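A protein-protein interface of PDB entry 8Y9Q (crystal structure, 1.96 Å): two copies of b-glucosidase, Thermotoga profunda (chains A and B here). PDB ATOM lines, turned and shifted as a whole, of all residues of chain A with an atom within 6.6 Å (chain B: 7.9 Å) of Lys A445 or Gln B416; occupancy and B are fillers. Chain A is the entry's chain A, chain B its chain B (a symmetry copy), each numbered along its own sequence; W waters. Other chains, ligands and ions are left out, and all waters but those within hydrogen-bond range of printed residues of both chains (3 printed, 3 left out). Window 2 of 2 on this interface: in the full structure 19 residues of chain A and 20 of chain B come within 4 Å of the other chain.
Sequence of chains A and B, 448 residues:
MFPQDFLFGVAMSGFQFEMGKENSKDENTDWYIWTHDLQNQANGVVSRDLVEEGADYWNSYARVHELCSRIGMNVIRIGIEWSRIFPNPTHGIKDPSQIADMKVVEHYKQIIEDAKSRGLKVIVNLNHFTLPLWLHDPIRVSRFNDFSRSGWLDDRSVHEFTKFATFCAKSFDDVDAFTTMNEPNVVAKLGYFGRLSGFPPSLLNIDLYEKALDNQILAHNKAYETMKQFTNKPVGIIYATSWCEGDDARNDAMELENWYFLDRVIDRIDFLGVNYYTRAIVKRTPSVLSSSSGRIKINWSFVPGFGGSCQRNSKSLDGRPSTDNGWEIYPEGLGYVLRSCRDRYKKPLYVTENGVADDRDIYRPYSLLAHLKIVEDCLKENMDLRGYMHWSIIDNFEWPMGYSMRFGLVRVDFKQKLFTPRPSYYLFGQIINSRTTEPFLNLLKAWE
Printed residues of chain B that touch a printed residue of chain A: Asp B359, Arg B360, Arg B411, Asp B413 and Gln B416. Of the 8 printed residues of chain A, 4 touch a printed residue of chain B. Printed residues of chain A that touch a printed residue of chain B: Asn A442, Lys A445, Ala A446 and Trp A447. Hydrophobic or aromatic side chains of chain A within 4 Å of the printed part of chain B: Ala A446 and Trp A447.
The backbone NH (N) of Asp B413 sits at hydrogen-bond distance from the backbone carbonyl oxygen (O) of Leu B418 (2.8 Å). The side-chain carboxylate (OD1) of Asp B413 lies within hydrogen-bond range of the backbone NH (N) of Lys B415, 3.3 Å away. The side-chain carboxylate (OD2) of Asp B413 sits close to the side-chain amide oxygen (OE1) of Gln B416 (2.9 Å). OD1 of Asp B359 is in salt-bridge range of NE of Arg B411 (2.8 Å). The guanidinium group of Arg B406 lies within salt-bridge range of the side-chain carboxylate of Asp B359 (3.9 Å).
Lys A445 touches just these residues of chain B: Arg B411, Asp B413 and Gln B416. Printed residues of chain A within 4 Å of Gln B416: Asn A442 and Lys A445. Of chain B, only Asp B359 (3.3 Å) and Arg B360 (3.0 Å) come within 4 Å of Ala A446. Printed residues of chain B within 4 Å of Asn A442: Arg B411, Asp B413 and Gln B416. Of the printed residues of chain B, Trp A447 touches Arg B360. Of the printed residues of chain A, Asp B413 touches Asn A442 and Lys A445. Leu A441 touches none of the printed residues of chain B. The nearest residue of chain B that does not touch Lys A445 is Asp B359 (4.9 Å). The nearest printed residue of chain B that does not touch Asn A442 is Val B412 (4.2 Å).
The side-chain carboxylate (OD2) of Asp B413 lies within hydrogen-bond range of the side-chain amide nitrogen (ND2) of Asn A442, at 3.0 Å. OD1 of Asn A442 is in hydrogen-bond range of NH1 of Arg B411, 2.9 Å away. NE of Arg B360 sits at hydrogen-bond distance from O of Ala A446, at 3.0 Å. The side-chain amino group (NZ) of Lys A445 lies within salt-bridge range of the side-chain carboxylate (OD2) of Asp B413 (2.9 Å).
No position is printed for both chains. Of the 9 pairs that touch across the chains among the printed residues, none has its exchanged pair printed and touching as well.
Water W3 lies within hydrogen-bond range of O of Glu A448 (2.6 Å) and NH2 of Arg B360 (3.3 Å). Water W1 bridges O of Asp B359 (2.9 Å) and O of Leu A443 (3.0 Å). Water W2 lies within hydrogen-bond range of ND2 of Asn A442 and OE1 of Gln B416.
OE1 of Gln B416 touches ND2 of Asn A442, at 3.8 Å. Lys A445 touches Arg B411 (CB to NH1, 3.9 Å). OE1 of Gln B416 touches NZ of Lys A445 (3.5 Å). Asp B359 touches Ala A446 (OD2 to CB, 3.3 Å). CD of Arg B360 touches CD2 of Trp A447, at 3.7 Å.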
ATOM      1  N   LEU A 441      14.892  -5.538  -8.503  1.00  0.00           N
ATOM      2  CA  LEU A 441      14.810  -6.447  -7.366  1.00  0.00           C
ATOM      3  C   LEU A 441      13.489  -7.203  -7.301  1.00  0.00           C
ATOM      4  O   LEU A 441      13.447  -8.306  -6.751  1.00  0.00           O
ATOM      5  CB  LEU A 441      15.015  -5.655  -6.072  1.00  0.00           C
ATOM      6  CG  LEU A 441      16.415  -5.066  -5.880  1.00  0.00           C
ATOM      7  CD1 LEU A 441      16.555  -4.499  -4.483  1.00  0.00           C
ATOM      8  CD2 LEU A 441      17.477  -6.130  -6.128  1.00  0.00           C
ATOM      9  N   ASN A 442      12.397  -6.625  -7.812  1.00  0.00           N
ATOM     10  CA  ASN A 442      11.106  -7.301  -7.675  1.00  0.00           C
ATOM     11  C   ASN A 442      11.079  -8.642  -8.398  1.00  0.00           C
ATOM     12  O   ASN A 442      10.299  -9.529  -8.024  1.00  0.00           O
ATOM     13  CB  ASN A 442       9.961  -6.438  -8.209  1.00  0.00           C
ATOM     14  CG  ASN A 442       8.602  -6.898  -7.675  1.00  0.00           C
ATOM     15  OD1 ASN A 442       7.692  -7.214  -8.446  1.00  0.00           O
ATOM     16  ND2 ASN A 442       8.448  -6.886  -6.352  1.00  0.00           N
ATOM     17  N   LEU A 443      11.899  -8.805  -9.448  1.00  0.00           N
ATOM     18  CA  LEU A 443      11.973 -10.089 -10.152  1.00  0.00           C
ATOM     19  C   LEU A 443      12.359 -11.222  -9.211  1.00  0.00           C
ATOM     20  O   LEU A 443      11.965 -12.377  -9.429  1.00  0.00           O
ATOM     21  CB  LEU A 443      12.982 -10.022 -11.306  1.00  0.00           C
ATOM     22  CG  LEU A 443      12.673  -9.042 -12.445  1.00  0.00           C
ATOM     23  CD1 LEU A 443      13.714  -9.139 -13.553  1.00  0.00           C
ATOM     24  CD2 LEU A 443      11.248  -9.263 -12.995  1.00  0.00           C
ATOM     25  N   LEU A 444      13.139 -10.909  -8.174  1.00  0.00           N
ATOM     26  CA  LEU A 444      13.612 -11.921  -7.243  1.00  0.00           C
ATOM     27  C   LEU A 444      12.456 -12.531  -6.468  1.00  0.00           C
ATOM     28  O   LEU A 444      12.561 -13.663  -5.987  1.00  0.00           O
ATOM     29  CB  LEU A 444      14.617 -11.284  -6.284  1.00  0.00           C
ATOM     30  CG  LEU A 444      15.922 -10.845  -6.955  1.00  0.00           C
ATOM     31  CD1 LEU A 444      16.931 -10.452  -5.907  1.00  0.00           C
ATOM     32  CD2 LEU A 444      16.484 -11.961  -7.836  1.00  0.00           C
ATOM     33  N   LYS A 445      11.347 -11.795  -6.335  1.00  0.00           N
ATOM     34  CA  LYS A 445      10.220 -12.302  -5.567  1.00  0.00           C
ATOM     35  C   LYS A 445       9.607 -13.546  -6.198  1.00  0.00           C
ATOM     36  O   LYS A 445       8.997 -14.350  -5.483  1.00  0.00           O
ATOM     37  CB  LYS A 445       9.153 -11.217  -5.408  1.00  0.00           C
ATOM     38  CG  LYS A 445       9.450 -10.187  -4.307  1.00  0.00           C
ATOM     39  CD  LYS A 445       8.161  -9.455  -3.935  1.00  0.00           C
ATOM     40  CE  LYS A 445       8.360  -8.418  -2.842  1.00  0.00           C
ATOM     41  NZ  LYS A 445       7.064  -7.728  -2.534  1.00  0.00           N
ATOM     42  N   ALA A 446       9.767 -13.737  -7.514  1.00  0.00           N
ATOM     43  CA  ALA A 446       9.212 -14.925  -8.154  1.00  0.00           C
ATOM     44  C   ALA A 446       9.882 -16.208  -7.677  1.00  0.00           C
ATOM     45  O   ALA A 446       9.317 -17.291  -7.853  1.00  0.00           O
ATOM     46  CB  ALA A 446       9.336 -14.805  -9.674  1.00  0.00           C
ATOM     47  N   TRP A 447      11.064 -16.105  -7.079  1.00  0.00           N
ATOM     48  CA  TRP A 447      11.832 -17.255  -6.635  1.00  0.00           C
ATOM     49  C   TRP A 447      11.730 -17.491  -5.134  1.00  0.00           C
ATOM     50  O   TRP A 447      12.263 -18.490  -4.643  1.00  0.00           O
ATOM     51  CB  TRP A 447      13.298 -17.089  -7.060  1.00  0.00           C
ATOM     52  CG  TRP A 447      13.459 -17.019  -8.572  1.00  0.00           C
ATOM     53  CD1 TRP A 447      13.286 -15.923  -9.380  1.00  0.00           C
ATOM     54  CD2 TRP A 447      13.793 -18.108  -9.440  1.00  0.00           C
ATOM     55  NE1 TRP A 447      13.505 -16.272 -10.700  1.00  0.00           N
ATOM     56  CE2 TRP A 447      13.823 -17.604 -10.757  1.00  0.00           C
ATOM     57  CE3 TRP A 447      14.084 -19.459  -9.226  1.00  0.00           C
ATOM     58  CZ2 TRP A 447      14.124 -18.408 -11.856  1.00  0.00           C
ATOM     59  CZ3 TRP A 447      14.390 -20.258 -10.319  1.00  0.00           C
ATOM     60  CH2 TRP A 447      14.402 -19.732 -11.617  1.00  0.00           C
ATOM     61  N   GLU A 448      11.041 -16.620  -4.397  1.00  0.00           N
ATOM     62  CA  GLU A 448      10.728 -16.903  -2.994  1.00  0.00           C
ATOM     63  C   GLU A 448       9.226 -17.082  -2.756  1.00  0.00           C
ATOM     64  O   GLU A 448       8.754 -18.199  -2.525  1.00  0.00           O
ATOM     65  CB  GLU A 448      11.269 -15.805  -2.078  1.00  0.00           C
ATOM     66  CG  GLU A 448      11.314 -16.234  -0.611  1.00  0.00           C
ATOM     67  CD  GLU A 448      12.207 -17.447  -0.376  1.00  0.00           C
ATOM     68  OE1 GLU A 448      13.402 -17.393  -0.746  1.00  0.00           O
ATOM     69  OE2 GLU A 448      11.708 -18.455   0.179  1.00  0.00           O
ATOM     70  N   LYS B  21      -7.070   1.578  -7.737  1.00  0.00           N
ATOM     71  CA  LYS B  21      -7.230   2.814  -6.982  1.00  0.00           C
ATOM     72  C   LYS B  21      -8.714   3.050  -6.767  1.00  0.00           C
ATOM     73  O   LYS B  21      -9.530   2.711  -7.628  1.00  0.00           O
ATOM     74  CB  LYS B  21      -6.650   4.024  -7.729  1.00  0.00           C
ATOM     75  CG  LYS B  21      -5.157   4.193  -7.678  1.00  0.00           C
ATOM     76  CD  LYS B  21      -4.625   4.269  -6.272  1.00  0.00           C
ATOM     77  CE  LYS B  21      -3.505   3.256  -6.083  1.00  0.00           C
ATOM     78  NZ  LYS B  21      -2.254   3.684  -6.788  1.00  0.00           N
ATOM     79  N   GLU B  53      -7.633  -4.332  -6.036  1.00  0.00           N
ATOM     80  CA  GLU B  53      -6.250  -4.100  -5.626  1.00  0.00           C
ATOM     81  C   GLU B  53      -5.253  -4.393  -6.749  1.00  0.00           C
ATOM     82  O   GLU B  53      -4.095  -4.718  -6.480  1.00  0.00           O
ATOM     83  CB  GLU B  53      -5.910  -4.941  -4.394  1.00  0.00           C
ATOM     84  CG  GLU B  53      -6.921  -4.806  -3.255  1.00  0.00           C
ATOM     85  CD  GLU B  53      -6.386  -5.337  -1.927  1.00  0.00           C
ATOM     86  OE1 GLU B  53      -5.897  -6.498  -1.901  1.00  0.00           O
ATOM     87  OE2 GLU B  53      -6.494  -4.618  -0.912  1.00  0.00           O
ATOM     88  N   GLY B  54      -5.666  -4.243  -8.003  1.00  0.00           N
ATOM     89  CA  GLY B  54      -4.862  -4.640  -9.154  1.00  0.00           C
ATOM     90  C   GLY B  54      -3.903  -3.583  -9.667  1.00  0.00           C
ATOM     91  O   GLY B  54      -3.440  -2.713  -8.924  1.00  0.00           O
ATOM     92  N   ARG B  63       2.272   4.906 -18.052  1.00  0.00           N
ATOM     93  CA  ARG B  63       3.394   4.020 -17.740  1.00  0.00           C
ATOM     94  C   ARG B  63       3.316   2.730 -18.545  1.00  0.00           C
ATOM     95  O   ARG B  63       4.332   2.250 -19.058  1.00  0.00           O
ATOM     96  CB  ARG B  63       3.442   3.693 -16.236  1.00  0.00           C
ATOM     97  CG  ARG B  63       4.131   4.726 -15.350  1.00  0.00           C
ATOM     98  CD  ARG B  63       4.414   4.160 -13.922  1.00  0.00           C
ATOM     99  NE  ARG B  63       3.206   3.784 -13.192  1.00  0.00           N
ATOM    100  CZ  ARG B  63       3.127   2.825 -12.272  1.00  0.00           C
ATOM    101  NH1 ARG B  63       4.168   2.065 -11.966  1.00  0.00           N
ATOM    102  NH2 ARG B  63       1.972   2.624 -11.642  1.00  0.00           N
ATOM    103  N   ASP B 359       5.802 -16.728 -13.693  1.00  0.00           N
ATOM    104  CA  ASP B 359       6.307 -15.620 -12.877  1.00  0.00           C
ATOM    105  C   ASP B 359       7.830 -15.507 -12.970  1.00  0.00           C
ATOM    106  O   ASP B 359       8.384 -14.399 -13.018  1.00  0.00           O
ATOM    107  CB  ASP B 359       5.862 -15.819 -11.424  1.00  0.00           C
ATOM    108  CG  ASP B 359       6.098 -14.594 -10.553  1.00  0.00           C
ATOM    109  OD1 ASP B 359       6.381 -13.501 -11.082  1.00  0.00           O
ATOM    110  OD2 ASP B 359       6.022 -14.728  -9.316  1.00  0.00           O
ATOM    111  N   ARG B 360       8.525 -16.643 -13.008  1.00  0.00           N
ATOM    112  CA  ARG B 360       9.986 -16.644 -13.007  1.00  0.00           C
ATOM    113  C   ARG B 360      10.590 -16.328 -14.366  1.00  0.00           C
ATOM    114  O   ARG B 360      11.811 -16.150 -14.440  1.00  0.00           O
ATOM    115  CB  ARG B 360      10.492 -18.008 -12.526  1.00  0.00           C
ATOM    116  CG  ARG B 360       9.960 -18.379 -11.142  1.00  0.00           C
ATOM    117  CD  ARG B 360      10.643 -19.611 -10.559  1.00  0.00           C
ATOM    118  NE  ARG B 360      10.339 -19.744  -9.138  1.00  0.00           N
ATOM    119  CZ  ARG B 360      10.628 -20.806  -8.396  1.00  0.00           C
ATOM    120  NH1 ARG B 360      11.247 -21.862  -8.908  1.00  0.00           N
ATOM    121  NH2 ARG B 360      10.276 -20.815  -7.109  1.00  0.00           N
ATOM    122  N   ARG B 406       0.658 -15.277 -13.655  1.00  0.00           N
ATOM    123  CA  ARG B 406       1.289 -14.028 -14.085  1.00  0.00           C
ATOM    124  C   ARG B 406       1.707 -14.157 -15.544  1.00  0.00           C
ATOM    125  O   ARG B 406       2.684 -14.844 -15.853  1.00  0.00           O
ATOM    126  CB  ARG B 406       2.477 -13.721 -13.168  1.00  0.00           C
ATOM    127  CG  ARG B 406       2.008 -13.319 -11.750  1.00  0.00           C
ATOM    128  CD  ARG B 406       3.127 -13.192 -10.730  1.00  0.00           C
ATOM    129  NE  ARG B 406       2.669 -12.679  -9.438  1.00  0.00           N
ATOM    130  CZ  ARG B 406       2.677 -11.396  -9.092  1.00  0.00           C
ATOM    131  NH1 ARG B 406       3.056 -10.451  -9.943  1.00  0.00           N
ATOM    132  NH2 ARG B 406       2.315 -11.055  -7.853  1.00  0.00           N
ATOM    133  N   ARG B 411       6.703  -7.806 -14.796  1.00  0.00           N
ATOM    134  CA  ARG B 411       6.157  -8.187 -13.501  1.00  0.00           C
ATOM    135  C   ARG B 411       5.477  -7.005 -12.834  1.00  0.00           C
ATOM    136  O   ARG B 411       5.963  -5.872 -12.903  1.00  0.00           O
ATOM    137  CB  ARG B 411       7.261  -8.715 -12.571  1.00  0.00           C
ATOM    138  CG  ARG B 411       6.701  -9.359 -11.280  1.00  0.00           C
ATOM    139  CD  ARG B 411       7.760 -10.191 -10.535  1.00  0.00           C
ATOM    140  NE  ARG B 411       7.131 -11.229  -9.725  1.00  0.00           N
ATOM    141  CZ  ARG B 411       6.577 -11.027  -8.538  1.00  0.00           C
ATOM    142  NH1 ARG B 411       6.608  -9.836  -7.949  1.00  0.00           N
ATOM    143  NH2 ARG B 411       5.953 -12.039  -7.934  1.00  0.00           N
ATOM    144  N   VAL B 412       4.365  -7.271 -12.153  1.00  0.00           N
ATOM    145  CA  VAL B 412       3.694  -6.256 -11.346  1.00  0.00           C
ATOM    146  C   VAL B 412       3.806  -6.638  -9.884  1.00  0.00           C
ATOM    147  O   VAL B 412       3.434  -7.754  -9.497  1.00  0.00           O
ATOM    148  CB  VAL B 412       2.214  -6.092 -11.724  1.00  0.00           C
ATOM    149  CG1 VAL B 412       1.586  -5.011 -10.830  1.00  0.00           C
ATOM    150  CG2 VAL B 412       2.070  -5.749 -13.193  1.00  0.00           C
ATOM    151  N   ASP B 413       4.251  -5.709  -9.056  1.00  0.00           N
ATOM    152  CA  ASP B 413       4.075  -5.892  -7.628  1.00  0.00           C
ATOM    153  C   ASP B 413       2.818  -5.112  -7.274  1.00  0.00           C
ATOM    154  O   ASP B 413       2.817  -3.870  -7.284  1.00  0.00           O
ATOM    155  CB  ASP B 413       5.282  -5.429  -6.824  1.00  0.00           C
ATOM    156  CG  ASP B 413       5.128  -5.751  -5.354  1.00  0.00           C
ATOM    157  OD1 ASP B 413       4.202  -5.234  -4.696  1.00  0.00           O
ATOM    158  OD2 ASP B 413       5.881  -6.654  -4.896  1.00  0.00           O
ATOM    159  N   PHE B 414       1.737  -5.842  -7.021  1.00  0.00           N
ATOM    160  CA  PHE B 414       0.435  -5.202  -6.921  1.00  0.00           C
ATOM    161  C   PHE B 414       0.337  -4.339  -5.666  1.00  0.00           C
ATOM    162  O   PHE B 414      -0.265  -3.263  -5.705  1.00  0.00           O
ATOM    163  CB  PHE B 414      -0.664  -6.269  -6.985  1.00  0.00           C
ATOM    164  CG  PHE B 414      -0.783  -6.926  -8.346  1.00  0.00           C
ATOM    165  CD1 PHE B 414      -1.398  -6.257  -9.399  1.00  0.00           C
ATOM    166  CD2 PHE B 414      -0.251  -8.195  -8.580  1.00  0.00           C
ATOM    167  CE1 PHE B 414      -1.497  -6.836 -10.666  1.00  0.00           C
ATOM    168  CE2 PHE B 414      -0.340  -8.787  -9.851  1.00  0.00           C
ATOM    169  CZ  PHE B 414      -0.971  -8.106 -10.891  1.00  0.00           C
ATOM    170  N   LYS B 415       0.958  -4.759  -4.564  1.00  0.00           N
ATOM    171  CA  LYS B 415       0.950  -3.938  -3.353  1.00  0.00           C
ATOM    172  C   LYS B 415       1.680  -2.613  -3.567  1.00  0.00           C
ATOM    173  O   LYS B 415       1.155  -1.546  -3.231  1.00  0.00           O
ATOM    174  CB  LYS B 415       1.575  -4.708  -2.193  1.00  0.00           C
ATOM    175  N   GLN B 416       2.893  -2.653  -4.120  1.00  0.00           N
ATOM    176  CA  GLN B 416       3.667  -1.432  -4.304  1.00  0.00           C
ATOM    177  C   GLN B 416       3.368  -0.709  -5.607  1.00  0.00           C
ATOM    178  O   GLN B 416       3.903   0.383  -5.817  1.00  0.00           O
ATOM    179  CB  GLN B 416       5.173  -1.710  -4.199  1.00  0.00           C
ATOM    180  CG  GLN B 416       5.581  -2.758  -3.167  1.00  0.00           C
ATOM    181  CD  GLN B 416       7.015  -3.250  -3.361  1.00  0.00           C
ATOM    182  OE1 GLN B 416       7.256  -4.420  -3.682  1.00  0.00           O
ATOM    183  NE2 GLN B 416       7.974  -2.338  -3.200  1.00  0.00           N
ATOM    184  N   LYS B 417       2.528  -1.276  -6.471  1.00  0.00           N
ATOM    185  CA  LYS B 417       2.165  -0.659  -7.751  1.00  0.00           C
ATOM    186  C   LYS B 417       3.415  -0.409  -8.603  1.00  0.00           C
ATOM    187  O   LYS B 417       3.619   0.673  -9.156  1.00  0.00           O
ATOM    188  CB  LYS B 417       1.364   0.629  -7.525  1.00  0.00           C
ATOM    189  CG  LYS B 417       0.102   0.394  -6.683  1.00  0.00           C
ATOM    190  CD  LYS B 417      -0.934  -0.509  -7.392  1.00  0.00           C
ATOM    191  CE  LYS B 417      -2.281  -0.532  -6.639  1.00  0.00           C
ATOM    192  NZ  LYS B 417      -2.771  -1.926  -6.327  1.00  0.00           N
ATOM    193  N   LEU B 418       4.252  -1.442  -8.703  1.00  0.00           N
ATOM    194  CA  LEU B 418       5.573  -1.384  -9.313  1.00  0.00           C
ATOM    195  C   LEU B 418       5.606  -2.279 -10.545  1.00  0.00           C
ATOM    196  O   LEU B 418       5.133  -3.417 -10.494  1.00  0.00           O
ATOM    197  CB  LEU B 418       6.637  -1.862  -8.314  1.00  0.00           C
ATOM    198  CG  LEU B 418       8.127  -1.858  -8.689  1.00  0.00           C
ATOM    199  CD1 LEU B 418       8.576  -0.552  -9.358  1.00  0.00           C
ATOM    200  CD2 LEU B 418       9.021  -2.258  -7.492  1.00  0.00           C
ATOM    201  N   PHE B 419       6.187  -1.776 -11.635  1.00  0.00           N
ATOM    202  CA  PHE B 419       6.343  -2.512 -12.888  1.00  0.00           C
ATOM    203  C   PHE B 419       7.825  -2.824 -13.093  1.00  0.00           C
ATOM    204  O   PHE B 419       8.661  -1.917 -13.044  1.00  0.00           O
ATOM    205  CB  PHE B 419       5.835  -1.684 -14.078  1.00  0.00           C
ATOM    206  CG  PHE B 419       4.344  -1.370 -14.059  1.00  0.00           C
ATOM    207  CD1 PHE B 419       3.443  -2.136 -13.345  1.00  0.00           C
ATOM    208  CD2 PHE B 419       3.869  -0.247 -14.732  1.00  0.00           C
ATOM    209  CE1 PHE B 419       2.077  -1.814 -13.338  1.00  0.00           C
ATOM    210  CE2 PHE B 419       2.515   0.089 -14.723  1.00  0.00           C
ATOM    211  CZ  PHE B 419       1.618  -0.689 -14.028  1.00  0.00           C
HETATM  212  O   HOH W   1      10.394 -12.575 -11.982  1.00  0.00           O
HETATM  213  O   HOH W   2      10.408  -5.601  -4.621  1.00  0.00           O
HETATM  214  O   HOH W   3       8.502 -19.108  -4.937  1.00  0.00           O
